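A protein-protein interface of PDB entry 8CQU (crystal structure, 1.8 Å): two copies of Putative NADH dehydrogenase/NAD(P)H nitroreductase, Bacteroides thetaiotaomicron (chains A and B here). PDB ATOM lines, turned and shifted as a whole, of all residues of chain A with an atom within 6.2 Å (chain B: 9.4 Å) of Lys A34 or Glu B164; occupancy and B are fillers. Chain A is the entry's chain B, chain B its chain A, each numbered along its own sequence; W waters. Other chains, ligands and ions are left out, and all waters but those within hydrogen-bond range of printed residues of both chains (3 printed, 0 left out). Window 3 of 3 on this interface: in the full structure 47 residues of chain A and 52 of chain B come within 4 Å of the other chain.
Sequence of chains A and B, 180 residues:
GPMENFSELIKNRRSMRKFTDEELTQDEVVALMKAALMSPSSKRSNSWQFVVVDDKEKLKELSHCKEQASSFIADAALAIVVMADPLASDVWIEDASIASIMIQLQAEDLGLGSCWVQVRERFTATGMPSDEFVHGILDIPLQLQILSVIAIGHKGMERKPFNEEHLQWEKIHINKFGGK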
ATOM      1  N   VAL A  29      -5.275 -27.554   1.713  1.00  0.00           N
ATOM      2  CA  VAL A  29      -6.709 -27.755   1.731  1.00  0.00           C
ATOM      3  C   VAL A  29      -7.250 -27.432   3.122  1.00  0.00           C
ATOM      4  O   VAL A  29      -8.158 -26.651   3.262  1.00  0.00           O
ATOM      5  CB  VAL A  29      -7.134 -29.164   1.300  1.00  0.00           C
ATOM      6  CG1 VAL A  29      -8.653 -29.281   1.388  1.00  0.00           C
ATOM      7  CG2 VAL A  29      -6.699 -29.532  -0.098  1.00  0.00           C
ATOM      8  N   VAL A  30      -6.606 -27.954   4.163  1.00  0.00           N
ATOM      9  CA  VAL A  30      -6.982 -27.642   5.539  1.00  0.00           C
ATOM     10  C   VAL A  30      -6.915 -26.129   5.832  1.00  0.00           C
ATOM     11  O   VAL A  30      -7.802 -25.580   6.524  1.00  0.00           O
ATOM     12  CB  VAL A  30      -6.118 -28.478   6.519  1.00  0.00           C
ATOM     13  CG1 VAL A  30      -6.253 -27.999   7.954  1.00  0.00           C
ATOM     14  CG2 VAL A  30      -6.471 -29.952   6.423  1.00  0.00           C
ATOM     15  N   ALA A  31      -5.850 -25.471   5.376  1.00  0.00           N
ATOM     16  CA  ALA A  31      -5.703 -24.039   5.600  1.00  0.00           C
ATOM     17  C   ALA A  31      -6.871 -23.238   4.996  1.00  0.00           C
ATOM     18  O   ALA A  31      -7.393 -22.258   5.606  1.00  0.00           O
ATOM     19  CB  ALA A  31      -4.374 -23.567   5.120  1.00  0.00           C
ATOM     20  N   LEU A  32      -7.343 -23.693   3.826  1.00  0.00           N
ATOM     21  CA  LEU A  32      -8.488 -23.045   3.185  1.00  0.00           C
ATOM     22  C   LEU A  32      -9.765 -23.202   3.997  1.00  0.00           C
ATOM     23  O   LEU A  32     -10.483 -22.202   4.188  1.00  0.00           O
ATOM     24  CB  LEU A  32      -8.691 -23.561   1.757  1.00  0.00           C
ATOM     25  CG  LEU A  32      -7.582 -23.197   0.768  1.00  0.00           C
ATOM     26  CD1 LEU A  32      -7.677 -24.073  -0.477  1.00  0.00           C
ATOM     27  CD2 LEU A  32      -7.624 -21.714   0.440  1.00  0.00           C
ATOM     28  N   MET A  33      -9.994 -24.420   4.479  1.00  0.00           N
ATOM     29  CA  MET A  33     -11.170 -24.720   5.281  1.00  0.00           C
ATOM     30  C   MET A  33     -11.124 -23.928   6.595  1.00  0.00           C
ATOM     31  O   MET A  33     -12.118 -23.367   7.000  1.00  0.00           O
ATOM     32  CB  MET A  33     -11.188 -26.211   5.619  1.00  0.00           C
ATOM     33  CG  MET A  33     -11.359 -27.175   4.464  1.00  0.00           C
ATOM     34  SD  MET A  33     -11.150 -28.915   5.022  1.00  0.00           S
ATOM     35  CE  MET A  33     -11.488 -29.814   3.500  1.00  0.00           C
ATOM     36  N   LYS A  34      -9.953 -23.881   7.262  1.00  0.00           N
ATOM     37  CA  LYS A  34      -9.795 -23.050   8.436  1.00  0.00           C
ATOM     38  C   LYS A  34     -10.078 -21.585   8.163  1.00  0.00           C
ATOM     39  O   LYS A  34     -10.727 -20.949   8.997  1.00  0.00           O
ATOM     40  CB  LYS A  34      -8.384 -23.195   9.024  1.00  0.00           C
ATOM     41  CG  LYS A  34      -8.134 -24.515   9.716  1.00  0.00           C
ATOM     42  CD  LYS A  34      -6.728 -24.601  10.263  1.00  0.00           C
ATOM     43  CE  LYS A  34      -6.592 -25.799  11.178  1.00  0.00           C
ATOM     44  NZ  LYS A  34      -5.192 -26.018  11.623  1.00  0.00           N
ATOM     45  N   ALA A  35      -9.596 -21.021   7.052  1.00  0.00           N
ATOM     46  CA  ALA A  35      -9.894 -19.624   6.781  1.00  0.00           C
ATOM     47  C   ALA A  35     -11.407 -19.391   6.730  1.00  0.00           C
ATOM     48  O   ALA A  35     -11.866 -18.415   7.294  1.00  0.00           O
ATOM     49  CB  ALA A  35      -9.262 -19.145   5.508  1.00  0.00           C
ATOM     50  N   ALA A  36     -12.151 -20.279   6.048  1.00  0.00           N
ATOM     51  CA  ALA A  36     -13.605 -20.192   5.921  1.00  0.00           C
ATOM     52  C   ALA A  36     -14.228 -20.196   7.308  1.00  0.00           C
ATOM     53  O   ALA A  36     -14.958 -19.270   7.638  1.00  0.00           O
ATOM     54  CB  ALA A  36     -14.122 -21.336   5.063  1.00  0.00           C
ATOM     55  N   LEU A  37     -13.840 -21.196   8.141  1.00  0.00           N
ATOM     56  CA  LEU A  37     -14.393 -21.391   9.473  1.00  0.00           C
ATOM     57  C   LEU A  37     -13.993 -20.290  10.470  1.00  0.00           C
ATOM     58  O   LEU A  37     -14.677 -20.139  11.473  1.00  0.00           O
ATOM     59  CB  LEU A  37     -13.948 -22.776   9.953  1.00  0.00           C
ATOM     60  CG  LEU A  37     -14.504 -23.970   9.184  1.00  0.00           C
ATOM     61  CD1 LEU A  37     -13.979 -25.281   9.769  1.00  0.00           C
ATOM     62  CD2 LEU A  37     -16.029 -23.932   9.228  1.00  0.00           C
ATOM     63  N   MET A  38     -12.951 -19.504  10.189  1.00  0.00           N
ATOM     64  CA  MET A  38     -12.558 -18.379  11.064  1.00  0.00           C
ATOM     65  C   MET A  38     -13.193 -17.051  10.646  1.00  0.00           C
ATOM     66  O   MET A  38     -12.839 -16.006  11.205  1.00  0.00           O
ATOM     67  CB  MET A  38     -11.027 -18.198  11.037  1.00  0.00           C
ATOM     68  CG  MET A  38     -10.399 -19.246  11.811  1.00  0.00           C
ATOM     69  SD  MET A  38      -8.600 -19.000  12.041  1.00  0.00           S
ATOM     70  CE  MET A  38      -8.401 -20.723  12.424  1.00  0.00           C
ATOM     71  N   SER A  39     -14.098 -17.054   9.643  1.00  0.00           N
ATOM     72  CA  SER A  39     -14.635 -15.812   9.121  1.00  0.00           C
ATOM     73  C   SER A  39     -15.457 -15.103  10.180  1.00  0.00           C
ATOM     74  O   SER A  39     -16.229 -15.772  10.873  1.00  0.00           O
ATOM     75  CB  SER A  39     -15.498 -16.065   7.863  1.00  0.00           C
ATOM     76  OG  SER A  39     -14.622 -16.524   6.860  1.00  0.00           O
ATOM     77  N   PHE B   6      -1.094 -13.995   6.088  1.00  0.00           N
ATOM     78  CA  PHE B   6      -2.537 -13.793   6.025  1.00  0.00           C
ATOM     79  C   PHE B   6      -3.228 -14.670   7.074  1.00  0.00           C
ATOM     80  O   PHE B   6      -4.089 -14.198   7.833  1.00  0.00           O
ATOM     81  CB  PHE B   6      -3.118 -14.107   4.646  1.00  0.00           C
ATOM     82  CG  PHE B   6      -4.597 -13.808   4.631  1.00  0.00           C
ATOM     83  CD1 PHE B   6      -5.031 -12.489   4.619  1.00  0.00           C
ATOM     84  CD2 PHE B   6      -5.528 -14.826   4.753  1.00  0.00           C
ATOM     85  CE1 PHE B   6      -6.384 -12.177   4.644  1.00  0.00           C
ATOM     86  CE2 PHE B   6      -6.885 -14.520   4.804  1.00  0.00           C
ATOM     87  CZ  PHE B   6      -7.313 -13.201   4.715  1.00  0.00           C
ATOM     88  N   SER B   7      -2.811 -15.933   7.040  1.00  0.00           N
ATOM     89  CA  SER B   7      -2.995 -16.952   8.059  1.00  0.00           C
ATOM     90  C   SER B   7      -3.008 -16.402   9.494  1.00  0.00           C
ATOM     91  O   SER B   7      -3.896 -16.768  10.242  1.00  0.00           O
ATOM     92  CB  SER B   7      -1.897 -17.944   7.862  1.00  0.00           C
ATOM     93  OG  SER B   7      -2.000 -18.962   8.804  1.00  0.00           O
ATOM     94  N   GLU B   8      -2.034 -15.550   9.885  1.00  0.00           N
ATOM     95  CA  GLU B   8      -1.947 -15.012  11.249  1.00  0.00           C
ATOM     96  C   GLU B   8      -2.781 -13.733  11.382  1.00  0.00           C
ATOM     97  O   GLU B   8      -3.291 -13.432  12.460  1.00  0.00           O
ATOM     98  CB  GLU B   8      -0.504 -14.670  11.645  1.00  0.00           C
ATOM     99  CG  GLU B   8       0.423 -15.866  11.741  1.00  0.00           C
ATOM    100  CD  GLU B   8       0.550 -16.502  13.119  1.00  0.00           C
ATOM    101  OE1 GLU B   8       1.638 -16.369  13.715  1.00  0.00           O
ATOM    102  OE2 GLU B   8      -0.411 -17.164  13.578  1.00  0.00           O
ATOM    103  N   ILE B  10      -5.816 -13.330   9.999  1.00  0.00           N
ATOM    104  CA  ILE B  10      -7.207 -13.721  10.307  1.00  0.00           C
ATOM    105  C   ILE B  10      -7.384 -14.418  11.667  1.00  0.00           C
ATOM    106  O   ILE B  10      -8.481 -14.390  12.248  1.00  0.00           O
ATOM    107  CB  ILE B  10      -7.754 -14.589   9.162  1.00  0.00           C
ATOM    108  CG1 ILE B  10      -7.030 -15.938   9.033  1.00  0.00           C
ATOM    109  CG2 ILE B  10      -7.698 -13.778   7.876  1.00  0.00           C
ATOM    110  CD1 ILE B  10      -7.435 -16.729   7.821  1.00  0.00           C
ATOM    111  N   LYS B  11      -6.322 -15.111  12.145  1.00  0.00           N
ATOM    112  CA  LYS B  11      -6.306 -15.712  13.479  1.00  0.00           C
ATOM    113  C   LYS B  11      -6.422 -14.618  14.547  1.00  0.00           C
ATOM    114  O   LYS B  11      -7.240 -14.699  15.465  1.00  0.00           O
ATOM    115  CB  LYS B  11      -5.036 -16.559  13.682  1.00  0.00           C
ATOM    116  CG  LYS B  11      -5.065 -17.901  12.946  1.00  0.00           C
ATOM    117  CD  LYS B  11      -3.710 -18.642  12.898  1.00  0.00           C
ATOM    118  CE  LYS B  11      -3.040 -18.754  14.257  1.00  0.00           C
ATOM    119  NZ  LYS B  11      -3.939 -19.337  15.292  1.00  0.00           N
ATOM    120  N   ASN B  12      -5.604 -13.583  14.385  1.00  0.00           N
ATOM    121  CA  ASN B  12      -5.488 -12.492  15.333  1.00  0.00           C
ATOM    122  C   ASN B  12      -6.551 -11.426  15.179  1.00  0.00           C
ATOM    123  O   ASN B  12      -6.624 -10.607  16.089  1.00  0.00           O
ATOM    124  CB  ASN B  12      -4.140 -11.766  15.236  1.00  0.00           C
ATOM    125  CG  ASN B  12      -2.988 -12.664  15.661  1.00  0.00           C
ATOM    126  OD1 ASN B  12      -3.157 -13.507  16.544  1.00  0.00           O
ATOM    127  ND2 ASN B  12      -1.825 -12.497  15.041  1.00  0.00           N
ATOM    128  N   PRO B 161      -6.654 -14.360  20.272  1.00  0.00           N
ATOM    129  CA  PRO B 161      -6.768 -14.917  18.924  1.00  0.00           C
ATOM    130  C   PRO B 161      -7.866 -15.985  18.906  1.00  0.00           C
ATOM    131  O   PRO B 161      -8.351 -16.452  19.945  1.00  0.00           O
ATOM    132  CB  PRO B 161      -5.429 -15.605  18.674  1.00  0.00           C
ATOM    133  CG  PRO B 161      -4.937 -15.969  20.112  1.00  0.00           C
ATOM    134  CD  PRO B 161      -5.474 -14.867  21.015  1.00  0.00           C
ATOM    135  N   PHE B 162      -8.223 -16.416  17.701  1.00  0.00           N
ATOM    136  CA  PHE B 162      -9.196 -17.470  17.490  1.00  0.00           C
ATOM    137  C   PHE B 162      -8.609 -18.789  18.005  1.00  0.00           C
ATOM    138  O   PHE B 162      -7.507 -19.161  17.627  1.00  0.00           O
ATOM    139  CB  PHE B 162      -9.551 -17.568  15.989  1.00  0.00           C
ATOM    140  CG  PHE B 162     -10.677 -18.529  15.692  1.00  0.00           C
ATOM    141  CD1 PHE B 162     -10.493 -19.903  15.695  1.00  0.00           C
ATOM    142  CD2 PHE B 162     -11.943 -18.055  15.333  1.00  0.00           C
ATOM    143  CE1 PHE B 162     -11.551 -20.774  15.463  1.00  0.00           C
ATOM    144  CE2 PHE B 162     -12.986 -18.921  15.029  1.00  0.00           C
ATOM    145  CZ  PHE B 162     -12.786 -20.285  15.101  1.00  0.00           C
ATOM    146  N   ASN B 163      -9.354 -19.503  18.853  1.00  0.00           N
ATOM    147  CA  ASN B 163      -8.921 -20.792  19.369  1.00  0.00           C
ATOM    148  C   ASN B 163      -9.406 -21.914  18.435  1.00  0.00           C
ATOM    149  O   ASN B 163     -10.588 -22.194  18.393  1.00  0.00           O
ATOM    150  CB  ASN B 163      -9.391 -21.018  20.808  1.00  0.00           C
ATOM    151  CG  ASN B 163      -8.916 -22.349  21.342  1.00  0.00           C
ATOM    152  OD1 ASN B 163      -8.313 -23.212  20.662  1.00  0.00           O
ATOM    153  ND2 ASN B 163      -9.106 -22.473  22.631  1.00  0.00           N
ATOM    154  N   GLU B 164      -8.472 -22.595  17.764  1.00  0.00           N
ATOM    155  CA  GLU B 164      -8.838 -23.531  16.724  1.00  0.00           C
ATOM    156  C   GLU B 164      -9.527 -24.760  17.278  1.00  0.00           C
ATOM    157  O   GLU B 164     -10.164 -25.494  16.508  1.00  0.00           O
ATOM    158  CB  GLU B 164      -7.630 -23.951  15.892  1.00  0.00           C
ATOM    159  CG  GLU B 164      -7.230 -22.819  15.007  1.00  0.00           C
ATOM    160  CD  GLU B 164      -5.996 -23.101  14.168  1.00  0.00           C
ATOM    161  OE1 GLU B 164      -5.230 -22.138  13.956  1.00  0.00           O
ATOM    162  OE2 GLU B 164      -5.794 -24.289  13.825  1.00  0.00           O
ATOM    163  N   GLU B 165      -9.485 -24.948  18.598  1.00  0.00           N
ATOM    164  CA  GLU B 165     -10.300 -26.011  19.172  1.00  0.00           C
ATOM    165  C   GLU B 165     -11.780 -25.847  18.804  1.00  0.00           C
ATOM    166  O   GLU B 165     -12.460 -26.875  18.777  1.00  0.00           O
ATOM    167  CB  GLU B 165     -10.190 -26.113  20.688  1.00  0.00           C
ATOM    168  CG  GLU B 165     -11.001 -27.303  21.205  1.00  0.00           C
ATOM    169  CD  GLU B 165     -10.689 -27.822  22.593  1.00  0.00           C
ATOM    170  OE1 GLU B 165      -9.816 -27.198  23.284  1.00  0.00           O
ATOM    171  OE2 GLU B 165     -11.301 -28.883  22.969  1.00  0.00           O
ATOM    172  N   HIS B 166     -12.230 -24.595  18.544  1.00  0.00           N
ATOM    173  CA  HIS B 166     -13.629 -24.217  18.361  1.00  0.00           C
ATOM    174  C   HIS B 166     -13.989 -24.041  16.879  1.00  0.00           C
ATOM    175  O   HIS B 166     -15.061 -23.535  16.572  1.00  0.00           O
ATOM    176  CB  HIS B 166     -13.903 -22.863  19.034  1.00  0.00           C
ATOM    177  CG  HIS B 166     -13.659 -23.009  20.498  1.00  0.00           C
ATOM    178  ND1 HIS B 166     -12.951 -22.086  21.237  1.00  0.00           N
ATOM    179  CD2 HIS B 166     -13.983 -24.021  21.339  1.00  0.00           C
ATOM    180  CE1 HIS B 166     -12.860 -22.540  22.488  1.00  0.00           C
ATOM    181  NE2 HIS B 166     -13.484 -23.708  22.575  1.00  0.00           N
ATOM    182  N   LEU B 167     -13.111 -24.478  15.969  1.00  0.00           N
ATOM    183  CA  LEU B 167     -13.450 -24.566  14.556  1.00  0.00           C
ATOM    184  C   LEU B 167     -14.660 -25.489  14.383  1.00  0.00           C
ATOM    185  O   LEU B 167     -14.666 -26.591  14.880  1.00  0.00           O
ATOM    186  CB  LEU B 167     -12.266 -25.173  13.789  1.00  0.00           C
ATOM    187  CG  LEU B 167     -11.069 -24.261  13.562  1.00  0.00           C
ATOM    188  CD1 LEU B 167      -9.861 -25.070  13.110  1.00  0.00           C
ATOM    189  CD2 LEU B 167     -11.417 -23.187  12.571  1.00  0.00           C
ATOM    190  N   GLN B 168     -15.622 -25.084  13.569  1.00  0.00           N
ATOM    191  CA  GLN B 168     -16.848 -25.857  13.415  1.00  0.00           C
ATOM    192  C   GLN B 168     -16.720 -26.739  12.181  1.00  0.00           C
ATOM    193  O   GLN B 168     -17.332 -26.445  11.112  1.00  0.00           O
ATOM    194  CB  GLN B 168     -18.029 -24.897  13.305  1.00  0.00           C
ATOM    195  CG  GLN B 168     -18.326 -24.196  14.611  1.00  0.00           C
ATOM    196  CD  GLN B 168     -19.204 -22.993  14.372  1.00  0.00           C
ATOM    197  OE1 GLN B 168     -18.825 -22.000  13.728  1.00  0.00           O
ATOM    198  NE2 GLN B 168     -20.418 -23.088  14.880  1.00  0.00           N
ATOM    199  N   TRP B 169     -15.987 -27.838  12.361  1.00  0.00           N
ATOM    200  CA  TRP B 169     -15.713 -28.781  11.281  1.00  0.00           C
ATOM    201  C   TRP B 169     -16.958 -29.450  10.682  1.00  0.00           C
ATOM    202  O   TRP B 169     -16.893 -29.873   9.546  1.00  0.00           O
ATOM    203  CB  TRP B 169     -14.750 -29.856  11.765  1.00  0.00           C
ATOM    204  CG  TRP B 169     -13.367 -29.327  11.920  1.00  0.00           C
ATOM    205  CD1 TRP B 169     -12.751 -29.090  13.111  1.00  0.00           C
ATOM    206  CD2 TRP B 169     -12.501 -28.807  10.900  1.00  0.00           C
ATOM    207  NE1 TRP B 169     -11.535 -28.525  12.890  1.00  0.00           N
ATOM    208  CE2 TRP B 169     -11.336 -28.362  11.548  1.00  0.00           C
ATOM    209  CE3 TRP B 169     -12.568 -28.717   9.504  1.00  0.00           C
ATOM    210  CZ2 TRP B 169     -10.230 -27.870  10.851  1.00  0.00           C
ATOM    211  CZ3 TRP B 169     -11.488 -28.220   8.813  1.00  0.00           C
ATOM    212  CH2 TRP B 169     -10.330 -27.788   9.482  1.00  0.00           C
ATOM    213  N   ILE B 172     -18.091 -28.248   7.246  1.00  0.00           N
ATOM    214  CA  ILE B 172     -17.343 -28.669   6.068  1.00  0.00           C
ATOM    215  C   ILE B 172     -17.891 -30.005   5.579  1.00  0.00           C
ATOM    216  O   ILE B 172     -17.929 -30.964   6.347  1.00  0.00           O
ATOM    217  CB  ILE B 172     -15.834 -28.821   6.384  1.00  0.00           C
ATOM    218  CG1 ILE B 172     -15.241 -27.523   6.918  1.00  0.00           C
ATOM    219  CG2 ILE B 172     -15.062 -29.346   5.150  1.00  0.00           C
ATOM    220  CD1 ILE B 172     -15.296 -26.342   5.987  1.00  0.00           C
HETATM  221  O   HOH W   1     -10.880 -13.692  11.145  1.00  0.00           O
HETATM  222  O   HOH W   2      -6.217 -26.687  14.472  1.00  0.00           O
HETATM  223  O   HOH W   3     -15.947 -22.253  13.021  1.00  0.00           O
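Met A33 touches Trp B169 (CB to CZ3, 3.8 Å).
CG2 of Ile B172 touches SD of Met A33, at 3.9 Å.
Lys A34 touches Leu B167.
Lys A34 touches Trp B169 (CG to CH2, 3.9 Å).
CD2 of Leu A37 touches O of Gln B168, at 3.4 Å.
Trp B169 touches Leu A37.
Ile B172 touches Leu A37 (CG1 to CD1, 3.8 Å).
SD of Met A38 touches CG of Lys B11 (3.8 Å).
Phe B162 touches Met A38.
CD2 of Leu B167 touches CE of Met A38, at 3.9 Å.
No position is printed for both chains.
Of the 14 pairs that touch across the chains among the printed residues, none has its exchanged pair printed and touching as well.
Of the 16 printed residues of chain B, 8 touch a printed residue of chain A.
Hydrophobic or aromatic side chains of chain B that line the printed part of chain A: Ile B10, Phe B162, Leu B167, Trp B169 and Ile B172.
Among the printed residues, 14 pairs touch across the chains.
Water W2 lies within hydrogen-bond range of OE2 of Glu B164 (2.5 Å) and NZ of Lys A34 (3.1 Å).
Water W1 bridges O of Ile B10 (2.7 Å) and O of Met A38 (3.0 Å).
Water W3 bridges N of Gln B168 and O of Leu A37.
Lys A34 touches three residues of chain B.
Of chain B, only Ile B10 comes within 4 Å of Ala A35.
Of the printed residues of chain B, Met A38 touches Lys B11, Phe B162, Glu B164 and Leu B167.
Printed residues of chain A within 4 Å of Lys B11: Met A38 (3.8 Å).
Glu B164 touches two residues of chain A.
Glu B165 touches none of the printed residues of chain A.
Of the printed residues of chain A, Trp B169 touches Met A33, Lys A34 and Leu A37.
The nearest printed residue of chain B that does not touch Met A33 is Leu B167 (5.6 Å).
The backbone carbonyl oxygen (O) of Lys B11 sits at hydrogen-bond distance from the backbone NH (N) of Phe B162, 3.0 Å away.
OG of Ser A39 lies within hydrogen-bond range of O of Ala A35 (3.4 Å).
NZ of Lys B11 is in salt-bridge range of OE1 of Glu B164, at 3.4 Å.
OE2 of Glu B164 is in salt-bridge range of NZ of Lys A34 (2.9 Å).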
